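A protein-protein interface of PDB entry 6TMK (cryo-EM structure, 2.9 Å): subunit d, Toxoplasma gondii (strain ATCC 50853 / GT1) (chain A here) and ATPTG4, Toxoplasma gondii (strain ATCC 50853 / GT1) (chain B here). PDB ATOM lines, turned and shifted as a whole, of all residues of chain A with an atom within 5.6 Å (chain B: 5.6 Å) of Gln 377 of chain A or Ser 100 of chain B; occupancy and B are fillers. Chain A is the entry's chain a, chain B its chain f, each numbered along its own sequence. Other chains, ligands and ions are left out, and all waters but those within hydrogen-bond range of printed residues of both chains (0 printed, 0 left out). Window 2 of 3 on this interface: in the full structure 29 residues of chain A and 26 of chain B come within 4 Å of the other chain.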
ATOM      1  N   ASP A 354      21.301  21.524  18.553  1.00  0.00           N
ATOM      2  CA  ASP A 354      21.992  22.418  19.468  1.00  0.00           C
ATOM      3  C   ASP A 354      21.657  23.882  19.226  1.00  0.00           C
ATOM      4  O   ASP A 354      22.239  24.753  19.878  1.00  0.00           O
ATOM      5  CB  ASP A 354      23.506  22.210  19.358  1.00  0.00           C
ATOM      6  CG  ASP A 354      24.229  22.483  20.661  1.00  0.00           C
ATOM      7  OD1 ASP A 354      25.414  22.108  20.772  1.00  0.00           O
ATOM      8  OD2 ASP A 354      23.614  23.073  21.573  1.00  0.00           O
ATOM      9  N   GLU A 375      26.969  20.739  21.903  1.00  0.00           N
ATOM     10  CA  GLU A 375      27.526  21.181  23.169  1.00  0.00           C
ATOM     11  C   GLU A 375      27.388  20.084  24.217  1.00  0.00           C
ATOM     12  O   GLU A 375      26.479  19.251  24.162  1.00  0.00           O
ATOM     13  CB  GLU A 375      26.823  22.452  23.645  1.00  0.00           C
ATOM     14  CG  GLU A 375      27.340  22.989  24.966  1.00  0.00           C
ATOM     15  CD  GLU A 375      26.877  24.406  25.240  1.00  0.00           C
ATOM     16  OE1 GLU A 375      27.021  25.263  24.343  1.00  0.00           O
ATOM     17  OE2 GLU A 375      26.369  24.662  26.351  1.00  0.00           O
ATOM     18  N   GLN A 376      28.308  20.095  25.182  1.00  0.00           N
ATOM     19  CA  GLN A 376      28.435  18.967  26.098  1.00  0.00           C
ATOM     20  C   GLN A 376      27.136  18.687  26.838  1.00  0.00           C
ATOM     21  O   GLN A 376      26.830  17.526  27.131  1.00  0.00           O
ATOM     22  CB  GLN A 376      29.559  19.238  27.097  1.00  0.00           C
ATOM     23  CG  GLN A 376      30.057  18.002  27.821  1.00  0.00           C
ATOM     24  CD  GLN A 376      31.243  18.293  28.716  1.00  0.00           C
ATOM     25  OE1 GLN A 376      31.922  19.307  28.557  1.00  0.00           O
ATOM     26  NE2 GLN A 376      31.495  17.404  29.668  1.00  0.00           N
ATOM     27  N   GLN A 377      26.357  19.724  27.142  1.00  0.00           N
ATOM     28  CA  GLN A 377      25.067  19.511  27.785  1.00  0.00           C
ATOM     29  C   GLN A 377      24.069  18.815  26.869  1.00  0.00           C
ATOM     30  O   GLN A 377      23.111  18.214  27.366  1.00  0.00           O
ATOM     31  CB  GLN A 377      24.486  20.843  28.261  1.00  0.00           C
ATOM     32  CG  GLN A 377      24.372  21.900  27.178  1.00  0.00           C
ATOM     33  CD  GLN A 377      23.347  22.964  27.514  1.00  0.00           C
ATOM     34  OE1 GLN A 377      22.928  23.097  28.663  1.00  0.00           O
ATOM     35  NE2 GLN A 377      22.933  23.723  26.508  1.00  0.00           N
ATOM     36  N   ARG A 378      24.267  18.881  25.554  1.00  0.00           N
ATOM     37  CA  ARG A 378      23.353  18.281  24.589  1.00  0.00           C
ATOM     38  C   ARG A 378      24.018  17.154  23.806  1.00  0.00           C
ATOM     39  O   ARG A 378      23.625  16.858  22.677  1.00  0.00           O
ATOM     40  CB  ARG A 378      22.816  19.343  23.630  1.00  0.00           C
ATOM     41  CG  ARG A 378      21.895  20.362  24.278  1.00  0.00           C
ATOM     42  CD  ARG A 378      20.669  19.719  24.905  1.00  0.00           C
ATOM     43  NE  ARG A 378      20.101  18.667  24.067  1.00  0.00           N
ATOM     44  CZ  ARG A 378      19.326  18.888  23.010  1.00  0.00           C
ATOM     45  NH1 ARG A 378      19.020  20.128  22.651  1.00  0.00           N
ATOM     46  NH2 ARG A 378      18.855  17.867  22.310  1.00  0.00           N
ATOM     47  N   ARG A 379      25.025  16.513  24.397  1.00  0.00           N
ATOM     48  CA  ARG A 379      25.640  15.324  23.825  1.00  0.00           C
ATOM     49  C   ARG A 379      24.967  14.037  24.290  1.00  0.00           C
ATOM     50  O   ARG A 379      25.600  12.975  24.281  1.00  0.00           O
ATOM     51  CB  ARG A 379      27.131  15.298  24.160  1.00  0.00           C
ATOM     52  CG  ARG A 379      27.941  16.294  23.357  1.00  0.00           C
ATOM     53  CD  ARG A 379      29.409  16.265  23.733  1.00  0.00           C
ATOM     54  NE  ARG A 379      30.138  17.389  23.158  1.00  0.00           N
ATOM     55  CZ  ARG A 379      31.397  17.692  23.454  1.00  0.00           C
ATOM     56  NH1 ARG A 379      32.074  16.960  24.326  1.00  0.00           N
ATOM     57  NH2 ARG A 379      31.979  18.734  22.881  1.00  0.00           N
ATOM     58  N   ASP A 380      23.702  14.109  24.687  1.00  0.00           N
ATOM     59  CA  ASP A 380      23.003  12.966  25.248  1.00  0.00           C
ATOM     60  C   ASP A 380      22.462  12.068  24.139  1.00  0.00           C
ATOM     61  O   ASP A 380      22.319  12.477  22.984  1.00  0.00           O
ATOM     62  CB  ASP A 380      21.857  13.428  26.148  1.00  0.00           C
ATOM     63  CG  ASP A 380      21.505  12.408  27.214  1.00  0.00           C
ATOM     64  OD1 ASP A 380      21.298  11.227  26.862  1.00  0.00           O
ATOM     65  OD2 ASP A 380      21.434  12.789  28.400  1.00  0.00           O
ATOM     66  N   ALA B  98      33.986  13.273  27.113  1.00  0.00           N
ATOM     67  CA  ALA B  98      33.261  14.508  27.397  1.00  0.00           C
ATOM     68  C   ALA B  98      31.824  14.362  26.921  1.00  0.00           C
ATOM     69  O   ALA B  98      31.517  14.560  25.743  1.00  0.00           O
ATOM     70  CB  ALA B  98      33.943  15.692  26.722  1.00  0.00           C
ATOM     71  N   VAL B  99      30.932  14.004  27.846  1.00  0.00           N
ATOM     72  CA  VAL B  99      29.527  13.775  27.551  1.00  0.00           C
ATOM     73  C   VAL B  99      28.691  14.462  28.621  1.00  0.00           C
ATOM     74  O   VAL B  99      29.174  14.791  29.706  1.00  0.00           O
ATOM     75  CB  VAL B  99      29.187  12.272  27.472  1.00  0.00           C
ATOM     76  CG1 VAL B  99      27.816  12.069  26.856  1.00  0.00           C
ATOM     77  CG2 VAL B  99      30.243  11.538  26.669  1.00  0.00           C
ATOM     78  N   SER B 100      27.416  14.682  28.293  1.00  0.00           N
ATOM     79  CA  SER B 100      26.525  15.391  29.204  1.00  0.00           C
ATOM     80  C   SER B 100      26.495  14.737  30.579  1.00  0.00           C
ATOM     81  O   SER B 100      26.392  15.424  31.601  1.00  0.00           O
ATOM     82  CB  SER B 100      25.118  15.442  28.611  1.00  0.00           C
ATOM     83  OG  SER B 100      24.563  14.142  28.514  1.00  0.00           O
ATOM     84  N   SER B 101      26.588  13.411  30.626  1.00  0.00           N
ATOM     85  CA  SER B 101      26.351  12.662  31.851  1.00  0.00           C
ATOM     86  C   SER B 101      27.600  12.516  32.709  1.00  0.00           C
ATOM     87  O   SER B 101      27.532  11.893  33.773  1.00  0.00           O
ATOM     88  CB  SER B 101      25.801  11.276  31.516  1.00  0.00           C
ATOM     89  OG  SER B 101      26.518  10.697  30.441  1.00  0.00           O
ATOM     90  N   ALA B 102      28.729  13.070  32.282  1.00  0.00           N
ATOM     91  CA  ALA B 102      29.958  12.992  33.062  1.00  0.00           C
ATOM     92  C   ALA B 102      29.986  14.074  34.134  1.00  0.00           C
ATOM     93  O   ALA B 102      28.950  14.441  34.685  1.00  0.00           O
ATOM     94  CB  ALA B 102      31.169  13.113  32.154  1.00  0.00           C
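Of chain B, only Ser 100 comes within 4 Å of Gln 377 of chain A.
Ser 100 of chain B touches just these residues of chain A: Gln 376, Gln 377 and Asp 380.
Printed residues of chain B within 4 Å of Asp 380 of chain A: Ser 100 (3.4 Å).
Of the printed residues of chain B, Arg 379 of chain A touches Ala 98 and Val 99.
Of the printed residues of chain A, Val 99 of chain B touches Gln 376 and Arg 379.
Ala 102 of chain B touches none of the printed residues of chain A.
Ser 101 of chain B touches none of the printed residues of chain A.
Among the printed residues, merely in contact across the chains: Gln 377 of chain A with Ser 100 of chain B and Arg 379 of chain A with Val 99 of chain B.
Printed residues of chain A that touch a printed residue of chain B: Gln 376, Gln 377, Arg 379 and Asp 380.
NH1 of Arg 379 of chain A is in hydrogen-bond range of O of Ala 98 of chain B, 2.8 Å away.
The backbone carbonyl oxygen (O) of Val 99 of chain B sits at hydrogen-bond distance from the side-chain amide nitrogen (NE2) of Gln 376 of chain A (3.5 Å).
The backbone carbonyl oxygen (O) of Gln 376 of chain A sits close to the backbone NH (N) of Ser 100 of chain B, at 3.1 Å.
The side-chain carboxylate (OD2) of Asp 380 of chain A lies within hydrogen-bond range of the side-chain hydroxyl (OG) of Ser 100 of chain B, at 3.4 Å.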
